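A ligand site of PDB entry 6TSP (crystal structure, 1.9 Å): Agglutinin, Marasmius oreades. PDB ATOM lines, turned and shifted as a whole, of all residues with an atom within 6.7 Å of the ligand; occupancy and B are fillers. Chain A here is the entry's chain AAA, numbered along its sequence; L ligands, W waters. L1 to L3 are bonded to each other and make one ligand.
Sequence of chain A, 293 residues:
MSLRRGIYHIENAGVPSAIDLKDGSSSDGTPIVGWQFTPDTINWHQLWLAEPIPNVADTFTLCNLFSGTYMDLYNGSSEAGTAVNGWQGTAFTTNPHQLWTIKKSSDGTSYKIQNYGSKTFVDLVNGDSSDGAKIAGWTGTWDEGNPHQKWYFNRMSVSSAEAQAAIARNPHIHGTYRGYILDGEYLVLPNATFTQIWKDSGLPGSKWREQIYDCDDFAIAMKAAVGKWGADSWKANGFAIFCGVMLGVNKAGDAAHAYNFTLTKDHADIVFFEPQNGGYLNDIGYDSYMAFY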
ATOM      1  N   HIS A   9     -22.289  31.053  -8.018  1.00  0.00           N
ATOM      2  CA  HIS A   9     -21.762  29.756  -7.596  1.00  0.00           C
ATOM      3  C   HIS A   9     -20.542  29.978  -6.687  1.00  0.00           C
ATOM      4  O   HIS A   9     -19.580  30.628  -7.127  1.00  0.00           O
ATOM      5  CB  HIS A   9     -21.413  28.901  -8.846  1.00  0.00           C
ATOM      6  CG  HIS A   9     -21.177  27.464  -8.538  1.00  0.00           C
ATOM      7  ND1 HIS A   9     -19.924  26.870  -8.697  1.00  0.00           N
ATOM      8  CD2 HIS A   9     -22.009  26.490  -8.093  1.00  0.00           C
ATOM      9  CE1 HIS A   9     -19.987  25.610  -8.303  1.00  0.00           C
ATOM     10  NE2 HIS A   9     -21.266  25.339  -7.996  1.00  0.00           N
ATOM     11  N   ASP A  20     -23.408  24.266  -0.890  1.00  0.00           N
ATOM     12  CA  ASP A  20     -24.445  23.344  -1.397  1.00  0.00           C
ATOM     13  C   ASP A  20     -25.536  23.186  -0.326  1.00  0.00           C
ATOM     14  O   ASP A  20     -25.187  22.845   0.832  1.00  0.00           O
ATOM     15  CB  ASP A  20     -23.843  21.985  -1.794  1.00  0.00           C
ATOM     16  CG  ASP A  20     -24.815  21.024  -2.495  1.00  0.00           C
ATOM     17  OD1 ASP A  20     -25.790  20.563  -1.819  1.00  0.00           O
ATOM     18  OD2 ASP A  20     -24.511  20.631  -3.648  1.00  0.00           O
ATOM     19  N   LEU A  21     -26.761  23.577  -0.647  1.00  0.00           N
ATOM     20  CA  LEU A  21     -27.926  23.276   0.206  1.00  0.00           C
ATOM     21  C   LEU A  21     -28.320  21.823  -0.004  1.00  0.00           C
ATOM     22  O   LEU A  21     -28.691  21.471  -1.158  1.00  0.00           O
ATOM     23  CB  LEU A  21     -29.084  24.222  -0.163  1.00  0.00           C
ATOM     24  CG  LEU A  21     -30.377  24.008   0.627  1.00  0.00           C
ATOM     25  CD1 LEU A  21     -30.108  24.125   2.113  1.00  0.00           C
ATOM     26  CD2 LEU A  21     -31.444  25.004   0.196  1.00  0.00           C
ATOM     27  N   LYS A  22     -28.131  20.976   1.017  1.00  0.00           N
ATOM     28  CA  LYS A  22     -28.067  19.499   0.844  1.00  0.00           C
ATOM     29  C   LYS A  22     -29.407  18.985   0.284  1.00  0.00           C
ATOM     30  O   LYS A  22     -30.480  19.372   0.839  1.00  0.00           O
ATOM     31  CB  LYS A  22     -27.730  18.782   2.154  1.00  0.00           C
ATOM     32  CG  LYS A  22     -27.116  17.409   1.968  1.00  0.00           C
ATOM     33  CD  LYS A  22     -26.693  16.718   3.238  1.00  0.00           C
ATOM     34  CE  LYS A  22     -26.095  15.355   2.964  1.00  0.00           C
ATOM     35  NZ  LYS A  22     -25.599  14.707   4.202  1.00  0.00           N
ATOM     36  N   ASP A  23     -29.347  18.301  -0.859  1.00  0.00           N
ATOM     37  CA  ASP A  23     -30.525  17.768  -1.594  1.00  0.00           C
ATOM     38  C   ASP A  23     -31.476  18.902  -1.992  1.00  0.00           C
ATOM     39  O   ASP A  23     -32.584  18.593  -2.502  1.00  0.00           O
ATOM     40  CB  ASP A  23     -31.267  16.714  -0.789  1.00  0.00           C
ATOM     41  CG  ASP A  23     -32.044  15.730  -1.644  1.00  0.00           C
ATOM     42  OD1 ASP A  23     -31.517  15.345  -2.718  1.00  0.00           O
ATOM     43  OD2 ASP A  23     -33.181  15.388  -1.276  1.00  0.00           O
ATOM     44  N   GLY A  24     -31.015  20.142  -1.902  1.00  0.00           N
ATOM     45  CA  GLY A  24     -31.794  21.312  -2.324  1.00  0.00           C
ATOM     46  C   GLY A  24     -33.128  21.393  -1.576  1.00  0.00           C
ATOM     47  O   GLY A  24     -34.026  22.100  -2.059  1.00  0.00           O
ATOM     48  N   VAL A  33     -23.491  22.625   3.018  1.00  0.00           N
ATOM     49  CA  VAL A  33     -22.291  21.760   3.061  1.00  0.00           C
ATOM     50  C   VAL A  33     -21.392  22.123   1.886  1.00  0.00           C
ATOM     51  O   VAL A  33     -21.919  22.641   0.867  1.00  0.00           O
ATOM     52  CB  VAL A  33     -22.663  20.251   3.038  1.00  0.00           C
ATOM     53  CG1 VAL A  33     -23.376  19.835   4.303  1.00  0.00           C
ATOM     54  CG2 VAL A  33     -23.488  19.884   1.794  1.00  0.00           C
ATOM     55  N   TRP A  35     -19.576  20.631  -1.464  1.00  0.00           N
ATOM     56  CA  TRP A  35     -19.895  19.581  -2.448  1.00  0.00           C
ATOM     57  C   TRP A  35     -19.201  19.893  -3.783  1.00  0.00           C
ATOM     58  O   TRP A  35     -19.203  21.072  -4.185  1.00  0.00           O
ATOM     59  CB  TRP A  35     -21.420  19.458  -2.618  1.00  0.00           C
ATOM     60  CG  TRP A  35     -21.853  18.091  -3.015  1.00  0.00           C
ATOM     61  CD1 TRP A  35     -21.705  17.505  -4.244  1.00  0.00           C
ATOM     62  CD2 TRP A  35     -22.429  17.097  -2.162  1.00  0.00           C
ATOM     63  NE1 TRP A  35     -22.221  16.239  -4.229  1.00  0.00           N
ATOM     64  CE2 TRP A  35     -22.661  15.945  -2.962  1.00  0.00           C
ATOM     65  CE3 TRP A  35     -22.799  17.069  -0.815  1.00  0.00           C
ATOM     66  CZ2 TRP A  35     -23.238  14.789  -2.452  1.00  0.00           C
ATOM     67  CZ3 TRP A  35     -23.356  15.906  -0.302  1.00  0.00           C
ATOM     68  CH2 TRP A  35     -23.585  14.792  -1.119  1.00  0.00           C
ATOM     69  N   GLN A  36     -18.674  18.863  -4.431  1.00  0.00           N
ATOM     70  CA  GLN A  36     -17.986  19.007  -5.713  1.00  0.00           C
ATOM     71  C   GLN A  36     -19.009  19.397  -6.776  1.00  0.00           C
ATOM     72  O   GLN A  36     -20.239  19.364  -6.460  1.00  0.00           O
ATOM     73  CB  GLN A  36     -17.237  17.695  -6.091  1.00  0.00           C
ATOM     74  CG  GLN A  36     -18.142  16.548  -6.515  1.00  0.00           C
ATOM     75  CD  GLN A  36     -17.354  15.297  -6.866  1.00  0.00           C
ATOM     76  OE1 GLN A  36     -16.653  15.259  -7.878  1.00  0.00           O
ATOM     77  NE2 GLN A  36     -17.350  14.321  -5.955  1.00  0.00           N
ATOM     78  N   PHE A  37     -18.553  19.970  -7.835  1.00  0.00           N
ATOM     79  CA  PHE A  37     -19.421  20.623  -8.845  1.00  0.00           C
ATOM     80  C   PHE A  37     -18.907  20.272 -10.239  1.00  0.00           C
ATOM     81  O   PHE A  37     -17.750  19.794 -10.370  1.00  0.00           O
ATOM     82  CB  PHE A  37     -19.454  22.129  -8.619  1.00  0.00           C
ATOM     83  CG  PHE A  37     -18.107  22.784  -8.507  1.00  0.00           C
ATOM     84  CD1 PHE A  37     -17.531  22.997  -7.274  1.00  0.00           C
ATOM     85  CD2 PHE A  37     -17.534  23.404  -9.613  1.00  0.00           C
ATOM     86  CE1 PHE A  37     -16.319  23.684  -7.164  1.00  0.00           C
ATOM     87  CE2 PHE A  37     -16.349  24.114  -9.492  1.00  0.00           C
ATOM     88  CZ  PHE A  37     -15.731  24.209  -8.277  1.00  0.00           C
ATOM     89  N   THR A  38     -19.750  20.449 -11.238  1.00  0.00           N
ATOM     90  CA  THR A  38     -19.359  20.294 -12.658  1.00  0.00           C
ATOM     91  C   THR A  38     -19.465  21.655 -13.354  1.00  0.00           C
ATOM     92  O   THR A  38     -20.538  22.250 -13.394  1.00  0.00           O
ATOM     93  CB  THR A  38     -20.231  19.221 -13.336  1.00  0.00           C
ATOM     94  OG1 THR A  38     -20.248  18.062 -12.508  1.00  0.00           O
ATOM     95  CG2 THR A  38     -19.748  18.863 -14.718  1.00  0.00           C
ATOM     96  N   PRO A  39     -18.359  22.174 -13.924  1.00  0.00           N
ATOM     97  CA  PRO A  39     -18.390  23.447 -14.647  1.00  0.00           C
ATOM     98  C   PRO A  39     -19.256  23.383 -15.912  1.00  0.00           C
ATOM     99  O   PRO A  39     -19.359  22.334 -16.496  1.00  0.00           O
ATOM    100  CB  PRO A  39     -16.912  23.689 -15.055  1.00  0.00           C
ATOM    101  CG  PRO A  39     -16.111  22.709 -14.182  1.00  0.00           C
ATOM    102  CD  PRO A  39     -17.050  21.555 -13.929  1.00  0.00           C
ATOM    103  N   THR A  41     -22.295  23.440 -16.221  1.00  0.00           N
ATOM    104  CA  THR A  41     -23.653  22.881 -16.002  1.00  0.00           C
ATOM    105  C   THR A  41     -24.465  23.858 -15.186  1.00  0.00           C
ATOM    106  O   THR A  41     -23.857  24.753 -14.539  1.00  0.00           O
ATOM    107  CB  THR A  41     -23.615  21.507 -15.313  1.00  0.00           C
ATOM    108  OG1 THR A  41     -23.171  21.711 -13.961  1.00  0.00           O
ATOM    109  CG2 THR A  41     -22.708  20.518 -15.998  1.00  0.00           C
ATOM    110  N   ILE A  42     -25.727  23.550 -15.012  1.00  0.00           N
ATOM    111  CA  ILE A  42     -26.518  24.018 -13.875  1.00  0.00           C
ATOM    112  C   ILE A  42     -26.176  23.136 -12.667  1.00  0.00           C
ATOM    113  O   ILE A  42     -26.484  21.940 -12.708  1.00  0.00           O
ATOM    114  CB  ILE A  42     -28.018  23.962 -14.225  1.00  0.00           C
ATOM    115  CG1 ILE A  42     -28.363  24.877 -15.401  1.00  0.00           C
ATOM    116  CG2 ILE A  42     -28.857  24.276 -13.001  1.00  0.00           C
ATOM    117  CD1 ILE A  42     -28.030  26.357 -15.163  1.00  0.00           C
ATOM    118  N   ASN A  43     -25.564  23.721 -11.645  1.00  0.00           N
ATOM    119  CA  ASN A  43     -25.361  23.030 -10.321  1.00  0.00           C
ATOM    120  C   ASN A  43     -26.563  23.332  -9.435  1.00  0.00           C
ATOM    121  O   ASN A  43     -26.600  24.437  -8.781  1.00  0.00           O
ATOM    122  CB  ASN A  43     -24.045  23.414  -9.673  1.00  0.00           C
ATOM    123  CG  ASN A  43     -22.854  22.971 -10.495  1.00  0.00           C
ATOM    124  OD1 ASN A  43     -22.493  21.793 -10.493  1.00  0.00           O
ATOM    125  ND2 ASN A  43     -22.281  23.906 -11.259  1.00  0.00           N
ATOM    126  N   TRP A  44     -27.521  22.420  -9.409  1.00  0.00           N
ATOM    127  CA  TRP A  44     -28.925  22.709  -9.084  1.00  0.00           C
ATOM    128  C   TRP A  44     -29.048  23.207  -7.625  1.00  0.00           C
ATOM    129  O   TRP A  44     -30.006  23.979  -7.331  1.00  0.00           O
ATOM    130  CB  TRP A  44     -29.774  21.480  -9.328  1.00  0.00           C
ATOM    131  CG  TRP A  44     -30.245  21.377 -10.731  1.00  0.00           C
ATOM    132  CD1 TRP A  44     -29.704  20.627 -11.731  1.00  0.00           C
ATOM    133  CD2 TRP A  44     -31.296  22.139 -11.336  1.00  0.00           C
ATOM    134  NE1 TRP A  44     -30.368  20.846 -12.901  1.00  0.00           N
ATOM    135  CE2 TRP A  44     -31.350  21.764 -12.691  1.00  0.00           C
ATOM    136  CE3 TRP A  44     -32.218  23.069 -10.853  1.00  0.00           C
ATOM    137  CZ2 TRP A  44     -32.290  22.294 -13.569  1.00  0.00           C
ATOM    138  CZ3 TRP A  44     -33.124  23.623 -11.724  1.00  0.00           C
ATOM    139  CH2 TRP A  44     -33.167  23.228 -13.063  1.00  0.00           C
ATOM    140  N   HIS A  45     -28.204  22.693  -6.721  1.00  0.00           N
ATOM    141  CA  HIS A  45     -28.335  22.952  -5.261  1.00  0.00           C
ATOM    142  C   HIS A  45     -27.333  24.019  -4.819  1.00  0.00           C
ATOM    143  O   HIS A  45     -27.296  24.341  -3.546  1.00  0.00           O
ATOM    144  CB  HIS A  45     -28.171  21.645  -4.474  1.00  0.00           C
ATOM    145  CG  HIS A  45     -29.166  20.610  -4.841  1.00  0.00           C
ATOM    146  ND1 HIS A  45     -28.954  19.255  -4.611  1.00  0.00           N
ATOM    147  CD2 HIS A  45     -30.355  20.704  -5.480  1.00  0.00           C
ATOM    148  CE1 HIS A  45     -29.991  18.573  -5.086  1.00  0.00           C
ATOM    149  NE2 HIS A  45     -30.832  19.439  -5.666  1.00  0.00           N
ATOM    150  N   GLN A  46     -26.645  24.641  -5.764  1.00  0.00           N
ATOM    151  CA  GLN A  46     -25.366  25.388  -5.499  1.00  0.00           C
ATOM    152  C   GLN A  46     -25.434  26.832  -6.066  1.00  0.00           C
ATOM    153  O   GLN A  46     -24.369  27.440  -6.256  1.00  0.00           O
ATOM    154  CB  GLN A  46     -24.189  24.638  -6.093  1.00  0.00           C
ATOM    155  CG  GLN A  46     -23.884  23.332  -5.403  1.00  0.00           C
ATOM    156  CD  GLN A  46     -22.753  22.570  -6.078  1.00  0.00           C
ATOM    157  OE1 GLN A  46     -22.131  23.062  -7.021  1.00  0.00           O
ATOM    158  NE2 GLN A  46     -22.469  21.363  -5.584  1.00  0.00           N
ATOM    159  N   PHE A  66     -32.771  27.377  -5.966  1.00  0.00           N
ATOM    160  CA  PHE A  66     -33.622  26.181  -6.141  1.00  0.00           C
ATOM    161  C   PHE A  66     -34.664  26.113  -5.014  1.00  0.00           C
ATOM    162  O   PHE A  66     -35.856  25.864  -5.314  1.00  0.00           O
ATOM    163  CB  PHE A  66     -32.773  24.914  -6.166  1.00  0.00           C
ATOM    164  CG  PHE A  66     -33.572  23.650  -6.365  1.00  0.00           C
ATOM    165  CD1 PHE A  66     -34.195  23.390  -7.589  1.00  0.00           C
ATOM    166  CD2 PHE A  66     -33.788  22.759  -5.305  1.00  0.00           C
ATOM    167  CE1 PHE A  66     -34.965  22.237  -7.752  1.00  0.00           C
ATOM    168  CE2 PHE A  66     -34.563  21.617  -5.477  1.00  0.00           C
ATOM    169  CZ  PHE A  66     -35.150  21.354  -6.704  1.00  0.00           C
ATOM    170  N   ASP A 131     -17.637  15.410  -0.087  1.00  0.00           N
ATOM    171  CA  ASP A 131     -19.038  15.762  -0.397  1.00  0.00           C
ATOM    172  C   ASP A 131     -19.877  15.646   0.888  1.00  0.00           C
ATOM    173  O   ASP A 131     -19.868  14.590   1.481  1.00  0.00           O
ATOM    174  CB  ASP A 131     -19.576  14.891  -1.525  1.00  0.00           C
ATOM    175  CG  ASP A 131     -18.975  15.222  -2.895  1.00  0.00           C
ATOM    176  OD1 ASP A 131     -18.437  16.313  -3.024  1.00  0.00           O
ATOM    177  OD2 ASP A 131     -18.995  14.339  -3.774  1.00  0.00           O
HETATM  178  C1  LIG L   1     -26.933  16.306  -9.044  1.00  0.00           C
HETATM  179  C2  LIG L   1     -26.957  15.167 -10.011  1.00  0.00           C
HETATM  180  C3  LIG L   1     -28.291  14.435  -9.967  1.00  0.00           C
HETATM  181  C4  LIG L   1     -29.466  15.417 -10.066  1.00  0.00           C
HETATM  182  C5  LIG L   1     -29.316  16.518  -9.025  1.00  0.00           C
HETATM  183  C6  LIG L   1     -30.448  17.564  -9.083  1.00  0.00           C
HETATM  184  O1  LIG L   1     -25.906  14.245  -9.674  1.00  0.00           O
HETATM  185  O2  LIG L   1     -28.323  13.538 -11.044  1.00  0.00           O
HETATM  186  O3  LIG L   1     -29.524  15.970 -11.368  1.00  0.00           O
HETATM  187  O4  LIG L   1     -28.059  17.168  -9.231  1.00  0.00           O
HETATM  188  C1  LG2 L   2     -27.549  15.951  -5.495  1.00  0.00           C
HETATM  189  C2  LG2 L   2     -26.874  16.665  -6.652  1.00  0.00           C
HETATM  190  C3  LG2 L   2     -25.403  17.031  -6.321  1.00  0.00           C
HETATM  191  C4  LG2 L   2     -25.378  17.803  -4.989  1.00  0.00           C
HETATM  192  C5  LG2 L   2     -26.103  16.935  -3.919  1.00  0.00           C
HETATM  193  C6  LG2 L   2     -26.071  17.541  -2.515  1.00  0.00           C
HETATM  194  O1  LG2 L   2     -28.911  15.774  -5.847  1.00  0.00           O
HETATM  195  O2  LG2 L   2     -26.926  15.824  -7.779  1.00  0.00           O
HETATM  196  O3  LG2 L   2     -24.886  17.753  -7.370  1.00  0.00           O
HETATM  197  O4  LG2 L   2     -25.957  19.125  -5.105  1.00  0.00           O
HETATM  198  O5  LG2 L   2     -27.463  16.731  -4.319  1.00  0.00           O
HETATM  199  O6  LG2 L   2     -27.157  18.492  -2.341  1.00  0.00           O
HETATM  200  C1  LG3 L   3     -23.579  18.183  -7.318  1.00  0.00           C
HETATM  201  C2  LG3 L   3     -23.157  18.959  -8.569  1.00  0.00           C
HETATM  202  C3  LG3 L   3     -22.940  18.012  -9.796  1.00  0.00           C
HETATM  203  C4  LG3 L   3     -22.071  16.842  -9.387  1.00  0.00           C
HETATM  204  C5  LG3 L   3     -22.704  16.165  -8.175  1.00  0.00           C
HETATM  205  C6  LG3 L   3     -21.965  14.882  -7.769  1.00  0.00           C
HETATM  206  O1  LG3 L   3     -24.151  19.935  -8.852  1.00  0.00           O
HETATM  207  O2  LG3 L   3     -22.340  18.721 -10.868  1.00  0.00           O
HETATM  208  O3  LG3 L   3     -20.721  17.279  -9.093  1.00  0.00           O
HETATM  209  O4  LG3 L   3     -22.682  17.076  -7.098  1.00  0.00           O
HETATM  210  O5  LG3 L   3     -22.545  14.376  -6.550  1.00  0.00           O
HETATM  211  O   HOH W   1     -24.239  19.810 -12.276  1.00  0.00           O
HETATM  212  O   HOH W   2     -25.126  13.310  -7.277  1.00  0.00           O
HETATM  213  O   HOH W   3     -26.078  20.838  -7.315  1.00  0.00           O
HETATM  214  O   HOH W   4     -26.520  19.742 -10.421  1.00  0.00           O
HETATM  215  O   HOH W   5     -31.833  16.377 -12.888  1.00  0.00           O
HETATM  216  O   HOH W   6     -28.771  14.984  -2.456  1.00  0.00           O
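The side-chain carboxylate of Asp 20 sits at hydrogen-bond distance from an oxygen (O6) of LG2 L2 (2.5 Å). O6 of LG2 L2 is in hydrogen-bond range of N of Asp 23 (2.7 Å). N of Thr 38 sits at hydrogen-bond distance from O2 of LG3 L3, 3.1 Å away. OG1 of Thr 38 lies within hydrogen-bond range of O2 of LG3 L3 (2.7 Å). A ring nitrogen (ND1) of His 45 is in hydrogen-bond range of an oxygen (O5) of LG2 L2 (2.9 Å). OD1 of Asn 43 sits at hydrogen-bond distance from O1 of LG3 L3 (3.0 Å). O5 of LG3 L3 is in hydrogen-bond range of NE1 of Trp 35 (3.0 Å). The backbone carbonyl oxygen (O) of Gln 36 lies within hydrogen-bond range of an oxygen (O3) of LG3 L3.
OD2 of Asp 20 is in hydrogen-bond range of NE2 of Gln 46. N of Val 33 is in hydrogen-bond range of O of Asp 20 (2.8 Å). N of Thr 38 sits at hydrogen-bond distance from OD1 of Asn 43, 3.1 Å away. O of Thr 38 is in hydrogen-bond range of OG1 of Thr 41. The backbone carbonyl oxygen of His 45 sits at hydrogen-bond distance from the backbone NH of Leu 21 (3.0 Å). O of Gln 36 sits at hydrogen-bond distance from NE2 of Gln 46 (3.1 Å). The side-chain amide nitrogen (NE2) of Gln 36 sits at hydrogen-bond distance from the side-chain carboxylate (OD2) of Asp 131 (2.7 Å). The side-chain amide oxygen (OE1) of Gln 46 lies within hydrogen-bond range of a ring nitrogen (NE2) of His 9.
Leu 21 touches the ligand. Lys 22 touches the ligand. Phe 37 touches the ligand. Trp 44 touches the ligand. Gln 46 touches the ligand. Hydrophobic or aromatic side chains that line the ligand: Trp 35, Trp 44 and His 45. Within 4 Å of the ligand: Asp 20, Leu 21, Lys 22, Asp 23, Trp 35, Gln 36, Phe 37, Thr 38, Asn 43, Trp 44, His 45 and Gln 46.
Water W1 lies within hydrogen-bond range of an oxygen (O2) of LG3 L3, the side-chain hydroxyl of Thr 41, the backbone carbonyl oxygen of Ile 42 and the side-chain amide oxygen of Asn 43. Water W3 lies within hydrogen-bond range of an oxygen (O1) of LG3 L3 (2.6 Å), the backbone NH of His 45 (2.9 Å) and the backbone NH of Trp 44 (3.0 Å). Water W4 lies within hydrogen-bond range of an oxygen (O1) of LG3 L3 (2.8 Å), the backbone NH (N) of Trp 44 (3.0 Å) and the backbone carbonyl oxygen (O) of Ile 42 (3.2 Å). Water W6 lies within hydrogen-bond range of OD1 of Asp 23 and O5 of LG2 L2.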
